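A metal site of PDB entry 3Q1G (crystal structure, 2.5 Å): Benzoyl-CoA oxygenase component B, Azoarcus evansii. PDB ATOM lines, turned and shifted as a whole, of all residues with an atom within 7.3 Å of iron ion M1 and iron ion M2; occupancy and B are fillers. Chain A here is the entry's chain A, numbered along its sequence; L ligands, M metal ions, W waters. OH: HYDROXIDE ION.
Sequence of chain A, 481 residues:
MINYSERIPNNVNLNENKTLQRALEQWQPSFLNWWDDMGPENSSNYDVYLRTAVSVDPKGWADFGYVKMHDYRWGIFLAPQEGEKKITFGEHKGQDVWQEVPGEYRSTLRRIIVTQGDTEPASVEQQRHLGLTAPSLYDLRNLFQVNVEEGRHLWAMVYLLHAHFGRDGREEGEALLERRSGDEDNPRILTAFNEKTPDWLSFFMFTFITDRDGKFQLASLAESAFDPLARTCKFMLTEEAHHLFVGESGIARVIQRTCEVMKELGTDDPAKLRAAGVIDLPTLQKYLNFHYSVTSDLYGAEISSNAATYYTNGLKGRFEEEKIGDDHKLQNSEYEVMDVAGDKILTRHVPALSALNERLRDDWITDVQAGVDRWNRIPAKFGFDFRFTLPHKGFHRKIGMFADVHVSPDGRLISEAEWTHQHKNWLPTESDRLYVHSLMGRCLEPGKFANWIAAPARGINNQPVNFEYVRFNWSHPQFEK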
ATOM      1  N   GLN A 116      -3.473 -17.566 -16.401  1.00  0.00           N
ATOM      2  CA  GLN A 116      -2.424 -16.528 -16.437  1.00  0.00           C
ATOM      3  C   GLN A 116      -1.108 -17.204 -16.765  1.00  0.00           C
ATOM      4  O   GLN A 116      -0.372 -16.735 -17.607  1.00  0.00           O
ATOM      5  CB  GLN A 116      -2.335 -15.766 -15.127  1.00  0.00           C
ATOM      6  CG  GLN A 116      -1.285 -14.703 -15.106  1.00  0.00           C
ATOM      7  CD  GLN A 116      -1.508 -13.625 -16.169  1.00  0.00           C
ATOM      8  OE1 GLN A 116      -2.576 -13.031 -16.242  1.00  0.00           O
ATOM      9  NE2 GLN A 116      -0.494 -13.392 -17.010  1.00  0.00           N
ATOM     10  N   THR A 119      -0.367 -18.101 -20.659  1.00  0.00           N
ATOM     11  CA  THR A 119      -0.034 -17.046 -21.612  1.00  0.00           C
ATOM     12  C   THR A 119       1.482 -16.773 -21.651  1.00  0.00           C
ATOM     13  O   THR A 119       2.010 -16.261 -22.645  1.00  0.00           O
ATOM     14  CB  THR A 119      -0.724 -15.704 -21.289  1.00  0.00           C
ATOM     15  OG1 THR A 119      -0.156 -15.164 -20.076  1.00  0.00           O
ATOM     16  CG2 THR A 119      -2.244 -15.856 -21.170  1.00  0.00           C
ATOM     17  N   GLU A 120       2.171 -17.121 -20.579  1.00  0.00           N
ATOM     18  CA  GLU A 120       3.588 -16.770 -20.428  1.00  0.00           C
ATOM     19  C   GLU A 120       4.462 -17.547 -21.403  1.00  0.00           C
ATOM     20  O   GLU A 120       5.097 -16.949 -22.260  1.00  0.00           O
ATOM     21  CB  GLU A 120       4.063 -16.933 -18.976  1.00  0.00           C
ATOM     22  CG  GLU A 120       3.122 -16.290 -17.917  1.00  0.00           C
ATOM     23  CD  GLU A 120       3.108 -14.759 -17.988  1.00  0.00           C
ATOM     24  OE1 GLU A 120       3.884 -14.180 -18.771  1.00  0.00           O
ATOM     25  OE2 GLU A 120       2.330 -14.162 -17.216  1.00  0.00           O
ATOM     26  N   SER A 123       3.735 -16.819 -25.145  1.00  0.00           N
ATOM     27  CA  SER A 123       4.394 -15.680 -25.818  1.00  0.00           C
ATOM     28  C   SER A 123       5.758 -16.043 -26.359  1.00  0.00           C
ATOM     29  O   SER A 123       6.126 -15.670 -27.479  1.00  0.00           O
ATOM     30  CB  SER A 123       4.474 -14.437 -24.926  1.00  0.00           C
ATOM     31  OG  SER A 123       5.354 -14.603 -23.807  1.00  0.00           O
ATOM     32  N   GLN A 127       7.078 -16.191 -30.324  1.00  0.00           N
ATOM     33  CA  GLN A 127       8.166 -15.278 -30.710  1.00  0.00           C
ATOM     34  C   GLN A 127       9.519 -15.956 -30.961  1.00  0.00           C
ATOM     35  O   GLN A 127      10.491 -15.258 -31.232  1.00  0.00           O
ATOM     36  CB  GLN A 127       8.341 -14.219 -29.624  1.00  0.00           C
ATOM     37  CG  GLN A 127       7.102 -13.362 -29.361  1.00  0.00           C
ATOM     38  CD  GLN A 127       7.176 -12.629 -28.056  1.00  0.00           C
ATOM     39  OE1 GLN A 127       6.179 -12.112 -27.565  1.00  0.00           O
ATOM     40  NE2 GLN A 127       8.376 -12.600 -27.471  1.00  0.00           N
ATOM     41  N   VAL A 146      12.674  -9.786 -22.926  1.00  0.00           N
ATOM     42  CA  VAL A 146      11.256 -10.114 -22.776  1.00  0.00           C
ATOM     43  C   VAL A 146      11.096 -11.629 -22.630  1.00  0.00           C
ATOM     44  O   VAL A 146      10.413 -12.095 -21.725  1.00  0.00           O
ATOM     45  CB  VAL A 146      10.405  -9.622 -23.951  1.00  0.00           C
ATOM     46  CG1 VAL A 146       8.966 -10.165 -23.842  1.00  0.00           C
ATOM     47  CG2 VAL A 146      10.412  -8.098 -24.021  1.00  0.00           C
ATOM     48  N   GLU A 149      12.008 -13.081 -19.192  1.00  0.00           N
ATOM     49  CA  GLU A 149      11.096 -12.616 -18.161  1.00  0.00           C
ATOM     50  C   GLU A 149       9.744 -13.311 -18.255  1.00  0.00           C
ATOM     51  O   GLU A 149       9.130 -13.660 -17.242  1.00  0.00           O
ATOM     52  CB  GLU A 149      10.961 -11.105 -18.239  1.00  0.00           C
ATOM     53  CG  GLU A 149      12.276 -10.423 -17.848  1.00  0.00           C
ATOM     54  CD  GLU A 149      12.188  -8.895 -17.824  1.00  0.00           C
ATOM     55  OE1 GLU A 149      11.185  -8.344 -18.346  1.00  0.00           O
ATOM     56  OE2 GLU A 149      13.134  -8.252 -17.295  1.00  0.00           O
ATOM     57  N   GLU A 150       9.284 -13.560 -19.471  1.00  0.00           N
ATOM     58  CA  GLU A 150       8.046 -14.359 -19.612  1.00  0.00           C
ATOM     59  C   GLU A 150       8.277 -15.783 -19.058  1.00  0.00           C
ATOM     60  O   GLU A 150       7.390 -16.367 -18.441  1.00  0.00           O
ATOM     61  CB  GLU A 150       7.518 -14.340 -21.030  1.00  0.00           C
ATOM     62  CG  GLU A 150       7.272 -12.912 -21.564  1.00  0.00           C
ATOM     63  CD  GLU A 150       6.067 -12.197 -20.954  1.00  0.00           C
ATOM     64  OE1 GLU A 150       5.538 -12.613 -19.861  1.00  0.00           O
ATOM     65  OE2 GLU A 150       5.680 -11.197 -21.580  1.00  0.00           O
ATOM     66  N   GLY A 151       9.499 -16.281 -19.238  1.00  0.00           N
ATOM     67  CA  GLY A 151       9.892 -17.515 -18.599  1.00  0.00           C
ATOM     68  C   GLY A 151       9.737 -17.397 -17.104  1.00  0.00           C
ATOM     69  O   GLY A 151       9.162 -18.278 -16.466  1.00  0.00           O
ATOM     70  N   HIS A 153       7.875 -15.482 -15.454  1.00  0.00           N
ATOM     71  CA  HIS A 153       6.474 -15.417 -15.101  1.00  0.00           C
ATOM     72  C   HIS A 153       5.853 -16.784 -15.035  1.00  0.00           C
ATOM     73  O   HIS A 153       4.984 -16.987 -14.213  1.00  0.00           O
ATOM     74  CB  HIS A 153       5.700 -14.542 -16.085  1.00  0.00           C
ATOM     75  CG  HIS A 153       6.076 -13.098 -15.985  1.00  0.00           C
ATOM     76  ND1 HIS A 153       5.532 -12.119 -16.787  1.00  0.00           N
ATOM     77  CD2 HIS A 153       6.975 -12.486 -15.183  1.00  0.00           C
ATOM     78  CE1 HIS A 153       6.052 -10.953 -16.450  1.00  0.00           C
ATOM     79  NE2 HIS A 153       6.946 -11.147 -15.499  1.00  0.00           N
ATOM     80  N   LEU A 154       6.300 -17.723 -15.884  1.00  0.00           N
ATOM     81  CA  LEU A 154       5.874 -19.107 -15.771  1.00  0.00           C
ATOM     82  C   LEU A 154       6.321 -19.694 -14.452  1.00  0.00           C
ATOM     83  O   LEU A 154       5.536 -20.368 -13.764  1.00  0.00           O
ATOM     84  CB  LEU A 154       6.406 -19.943 -16.925  1.00  0.00           C
ATOM     85  CG  LEU A 154       5.936 -21.417 -16.918  1.00  0.00           C
ATOM     86  CD1 LEU A 154       4.409 -21.490 -16.931  1.00  0.00           C
ATOM     87  CD2 LEU A 154       6.530 -22.181 -18.061  1.00  0.00           C
ATOM     88  N   PHE A 206       2.372  -6.474 -30.313  1.00  0.00           N
ATOM     89  CA  PHE A 206       2.001  -7.440 -29.308  1.00  0.00           C
ATOM     90  C   PHE A 206       2.455  -6.951 -27.947  1.00  0.00           C
ATOM     91  O   PHE A 206       1.651  -6.870 -27.005  1.00  0.00           O
ATOM     92  CB  PHE A 206       2.594  -8.797 -29.601  1.00  0.00           C
ATOM     93  CG  PHE A 206       2.100  -9.873 -28.709  1.00  0.00           C
ATOM     94  CD1 PHE A 206       1.069 -10.706 -29.101  1.00  0.00           C
ATOM     95  CD2 PHE A 206       2.686 -10.065 -27.451  1.00  0.00           C
ATOM     96  CE1 PHE A 206       0.611 -11.703 -28.249  1.00  0.00           C
ATOM     97  CE2 PHE A 206       2.230 -11.068 -26.591  1.00  0.00           C
ATOM     98  CZ  PHE A 206       1.188 -11.861 -26.963  1.00  0.00           C
ATOM     99  N   THR A 207       3.727  -6.600 -27.821  1.00  0.00           N
ATOM    100  CA  THR A 207       4.213  -6.196 -26.534  1.00  0.00           C
ATOM    101  C   THR A 207       3.614  -4.854 -26.160  1.00  0.00           C
ATOM    102  O   THR A 207       3.572  -4.513 -24.978  1.00  0.00           O
ATOM    103  CB  THR A 207       5.732  -6.136 -26.478  1.00  0.00           C
ATOM    104  OG1 THR A 207       6.184  -5.359 -27.572  1.00  0.00           O
ATOM    105  CG2 THR A 207       6.334  -7.472 -26.565  1.00  0.00           C
ATOM    106  N   THR A 210      -0.922  -6.428 -26.295  1.00  0.00           N
ATOM    107  CA  THR A 210      -1.309  -7.663 -25.643  1.00  0.00           C
ATOM    108  C   THR A 210      -0.620  -7.857 -24.300  1.00  0.00           C
ATOM    109  O   THR A 210      -1.252  -8.309 -23.346  1.00  0.00           O
ATOM    110  CB  THR A 210      -1.068  -8.861 -26.566  1.00  0.00           C
ATOM    111  OG1 THR A 210      -1.658  -8.569 -27.862  1.00  0.00           O
ATOM    112  CG2 THR A 210      -1.644 -10.115 -25.965  1.00  0.00           C
ATOM    113  N   ASP A 211       0.656  -7.509 -24.190  1.00  0.00           N
ATOM    114  CA  ASP A 211       1.298  -7.506 -22.877  1.00  0.00           C
ATOM    115  C   ASP A 211       0.557  -6.514 -21.970  1.00  0.00           C
ATOM    116  O   ASP A 211       0.553  -6.661 -20.744  1.00  0.00           O
ATOM    117  CB  ASP A 211       2.778  -7.128 -22.981  1.00  0.00           C
ATOM    118  CG  ASP A 211       3.669  -8.291 -23.443  1.00  0.00           C
ATOM    119  OD1 ASP A 211       3.502  -8.813 -24.574  1.00  0.00           O
ATOM    120  OD2 ASP A 211       4.567  -8.665 -22.654  1.00  0.00           O
ATOM    121  N   ARG A 212      -0.089  -5.501 -22.551  1.00  0.00           N
ATOM    122  CA  ARG A 212      -0.854  -4.566 -21.732  1.00  0.00           C
ATOM    123  C   ARG A 212      -2.093  -5.205 -21.109  1.00  0.00           C
ATOM    124  O   ARG A 212      -2.502  -4.827 -20.014  1.00  0.00           O
ATOM    125  CB  ARG A 212      -1.218  -3.327 -22.504  1.00  0.00           C
ATOM    126  CG  ARG A 212      -1.506  -2.121 -21.627  1.00  0.00           C
ATOM    127  CD  ARG A 212      -1.795  -0.931 -22.509  1.00  0.00           C
ATOM    128  NE  ARG A 212      -0.635  -0.656 -23.333  1.00  0.00           N
ATOM    129  CZ  ARG A 212       0.397   0.096 -22.951  1.00  0.00           C
ATOM    130  NH1 ARG A 212       0.414   0.691 -21.748  1.00  0.00           N
ATOM    131  NH2 ARG A 212       1.412   0.267 -23.775  1.00  0.00           N
ATOM    132  N   GLY A 214      -1.923  -8.206 -20.138  1.00  0.00           N
ATOM    133  CA  GLY A 214      -1.185  -8.752 -18.998  1.00  0.00           C
ATOM    134  C   GLY A 214      -1.200  -7.739 -17.867  1.00  0.00           C
ATOM    135  O   GLY A 214      -1.614  -8.065 -16.739  1.00  0.00           O
ATOM    136  N   LYS A 215      -0.781  -6.498 -18.152  1.00  0.00           N
ATOM    137  CA  LYS A 215      -0.713  -5.468 -17.122  1.00  0.00           C
ATOM    138  C   LYS A 215      -2.028  -5.462 -16.349  1.00  0.00           C
ATOM    139  O   LYS A 215      -2.055  -5.577 -15.105  1.00  0.00           O
ATOM    140  CB  LYS A 215      -0.427  -4.080 -17.733  1.00  0.00           C
ATOM    141  CG  LYS A 215      -0.458  -2.880 -16.726  1.00  0.00           C
ATOM    142  CD  LYS A 215      -0.365  -1.551 -17.455  1.00  0.00           C
ATOM    143  CE  LYS A 215      -0.437  -0.342 -16.534  1.00  0.00           C
ATOM    144  NZ  LYS A 215      -0.153   0.951 -17.318  1.00  0.00           N
ATOM    145  N   LEU A 218      -3.051  -8.647 -14.360  1.00  0.00           N
ATOM    146  CA  LEU A 218      -2.163  -8.742 -13.203  1.00  0.00           C
ATOM    147  C   LEU A 218      -2.464  -7.677 -12.145  1.00  0.00           C
ATOM    148  O   LEU A 218      -2.423  -7.969 -10.965  1.00  0.00           O
ATOM    149  CB  LEU A 218      -0.700  -8.594 -13.643  1.00  0.00           C
ATOM    150  CG  LEU A 218      -0.110  -9.739 -14.456  1.00  0.00           C
ATOM    151  CD1 LEU A 218       1.256  -9.310 -15.030  1.00  0.00           C
ATOM    152  CD2 LEU A 218       0.003 -11.053 -13.658  1.00  0.00           C
ATOM    153  N   MET A 236       5.434  -8.803 -10.770  1.00  0.00           N
ATOM    154  CA  MET A 236       5.344  -9.037 -12.181  1.00  0.00           C
ATOM    155  C   MET A 236       5.035  -7.745 -12.928  1.00  0.00           C
ATOM    156  O   MET A 236       5.559  -7.543 -14.015  1.00  0.00           O
ATOM    157  CB  MET A 236       4.312 -10.114 -12.487  1.00  0.00           C
ATOM    158  CG  MET A 236       4.757 -11.494 -12.062  1.00  0.00           C
ATOM    159  SD  MET A 236       3.486 -12.745 -12.125  1.00  0.00           S
ATOM    160  CE  MET A 236       3.165 -12.727 -13.897  1.00  0.00           C
ATOM    161  N   GLU A 239       7.986  -5.992 -14.178  1.00  0.00           N
ATOM    162  CA  GLU A 239       8.508  -6.620 -15.378  1.00  0.00           C
ATOM    163  C   GLU A 239       7.659  -6.267 -16.607  1.00  0.00           C
ATOM    164  O   GLU A 239       8.188  -5.940 -17.678  1.00  0.00           O
ATOM    165  CB  GLU A 239       8.595  -8.126 -15.193  1.00  0.00           C
ATOM    166  CG  GLU A 239       9.678  -8.514 -14.171  1.00  0.00           C
ATOM    167  CD  GLU A 239       9.520  -9.921 -13.611  1.00  0.00           C
ATOM    168  OE1 GLU A 239       8.391 -10.358 -13.303  1.00  0.00           O
ATOM    169  OE2 GLU A 239      10.560 -10.592 -13.447  1.00  0.00           O
ATOM    170  N   GLU A 240       6.337  -6.292 -16.435  1.00  0.00           N
ATOM    171  CA  GLU A 240       5.471  -5.969 -17.554  1.00  0.00           C
ATOM    172  C   GLU A 240       5.737  -4.553 -18.048  1.00  0.00           C
ATOM    173  O   GLU A 240       5.612  -4.298 -19.246  1.00  0.00           O
ATOM    174  CB  GLU A 240       4.008  -6.132 -17.202  1.00  0.00           C
ATOM    175  CG  GLU A 240       3.164  -6.427 -18.448  1.00  0.00           C
ATOM    176  CD  GLU A 240       3.384  -7.864 -19.005  1.00  0.00           C
ATOM    177  OE1 GLU A 240       4.194  -8.080 -19.897  1.00  0.00           O
ATOM    178  OE2 GLU A 240       2.728  -8.796 -18.587  1.00  0.00           O
ATOM    179  N   ALA A 241       6.112  -3.632 -17.148  1.00  0.00           N
ATOM    180  CA  ALA A 241       6.454  -2.269 -17.562  1.00  0.00           C
ATOM    181  C   ALA A 241       7.539  -2.250 -18.636  1.00  0.00           C
ATOM    182  O   ALA A 241       7.472  -1.458 -19.547  1.00  0.00           O
ATOM    183  CB  ALA A 241       6.864  -1.397 -16.362  1.00  0.00           C
ATOM    184  N   HIS A 242       8.532  -3.130 -18.527  1.00  0.00           N
ATOM    185  CA  HIS A 242       9.603  -3.206 -19.528  1.00  0.00           C
ATOM    186  C   HIS A 242       9.080  -3.684 -20.874  1.00  0.00           C
ATOM    187  O   HIS A 242       9.535  -3.201 -21.920  1.00  0.00           O
ATOM    188  CB  HIS A 242      10.773  -4.124 -19.112  1.00  0.00           C
ATOM    189  CG  HIS A 242      11.880  -4.197 -20.133  1.00  0.00           C
ATOM    190  ND1 HIS A 242      12.828  -3.200 -20.301  1.00  0.00           N
ATOM    191  CD2 HIS A 242      12.181  -5.147 -21.065  1.00  0.00           C
ATOM    192  CE1 HIS A 242      13.664  -3.532 -21.274  1.00  0.00           C
ATOM    193  NE2 HIS A 242      13.298  -4.703 -21.749  1.00  0.00           N
ATOM    194  N   HIS A 243       8.131  -4.592 -20.857  1.00  0.00           N
ATOM    195  CA  HIS A 243       7.612  -5.184 -22.071  1.00  0.00           C
ATOM    196  C   HIS A 243       6.838  -4.137 -22.847  1.00  0.00           C
ATOM    197  O   HIS A 243       6.978  -4.021 -24.071  1.00  0.00           O
ATOM    198  CB  HIS A 243       6.721  -6.405 -21.743  1.00  0.00           C
ATOM    199  CG  HIS A 243       7.431  -7.486 -20.960  1.00  0.00           C
ATOM    200  ND1 HIS A 243       6.810  -8.660 -20.569  1.00  0.00           N
ATOM    201  CD2 HIS A 243       8.712  -7.561 -20.516  1.00  0.00           C
ATOM    202  CE1 HIS A 243       7.679  -9.404 -19.898  1.00  0.00           C
ATOM    203  NE2 HIS A 243       8.839  -8.764 -19.856  1.00  0.00           N
ATOM    204  N   LEU A 244       6.034  -3.356 -22.134  1.00  0.00           N
ATOM    205  CA  LEU A 244       5.255  -2.280 -22.746  1.00  0.00           C
ATOM    206  C   LEU A 244       6.201  -1.241 -23.331  1.00  0.00           C
ATOM    207  O   LEU A 244       5.945  -0.705 -24.421  1.00  0.00           O
ATOM    208  CB  LEU A 244       4.344  -1.603 -21.734  1.00  0.00           C
ATOM    209  CG  LEU A 244       3.401  -2.548 -20.977  1.00  0.00           C
ATOM    210  CD1 LEU A 244       2.620  -1.734 -19.897  1.00  0.00           C
ATOM    211  CD2 LEU A 244       2.469  -3.314 -21.962  1.00  0.00           C
HETATM  212  O    OH L   1       5.000 -10.292 -19.085  1.00  0.00           O
HETATM  213 FE    FE M   1       4.836  -9.498 -20.957  1.00  0.00          FE
HETATM  214 FE    FE M   2       4.093 -12.031 -18.681  1.00  0.00          FE
HETATM  215  O   HOH W   1       2.915 -11.067 -21.078  1.00  0.00           O
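N of Asp 211 lies within hydrogen-bond range of O of Phe 206 (3.1 Å).
The side-chain amide nitrogen of Gln 116 lies within hydrogen-bond range of the side-chain carboxylate of Glu 120 (2.9 Å).
The side-chain hydroxyl (OG) of Ser 123 sits at hydrogen-bond distance from the backbone carbonyl oxygen (O) of Glu 120 (2.8 Å).
OE1 of Glu 149 is in hydrogen-bond range of NE2 of His 243, 2.8 Å away.
The side-chain carboxylate (OE1) of Glu 239 sits at hydrogen-bond distance from a ring nitrogen (NE2) of His 153, 2.7 Å away.
Of the 26 residues printed, 4 come within 4 Å of iron ion M2.
The nearest printed residue that does not touch iron ion M2 is His 243 (4.6 Å).
The nearest printed residue that does not touch iron ion M1 is His 153 (4.9 Å).
OE1 of Glu 150 is bound to iron ion M2 (2.0 Å).
Iron ion M2 is bound by O of the ligand.
Iron ion M2 is bound by the side-chain carboxylate (OE1) of Glu 120 (2.2 Å).
Iron ion M2 is bound by a ring nitrogen (ND1) of His 153.
Slightly farther from iron ion M2 lies water W1 (2.8 Å).
Iron ion M1 is bound by OE1 of Glu 240, OD2 of Asp 211, OE2 of Glu 150, O of the ligand, ND1 of His 243 and water W1.
Iron ion M1 has six donor atoms within binding distance.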
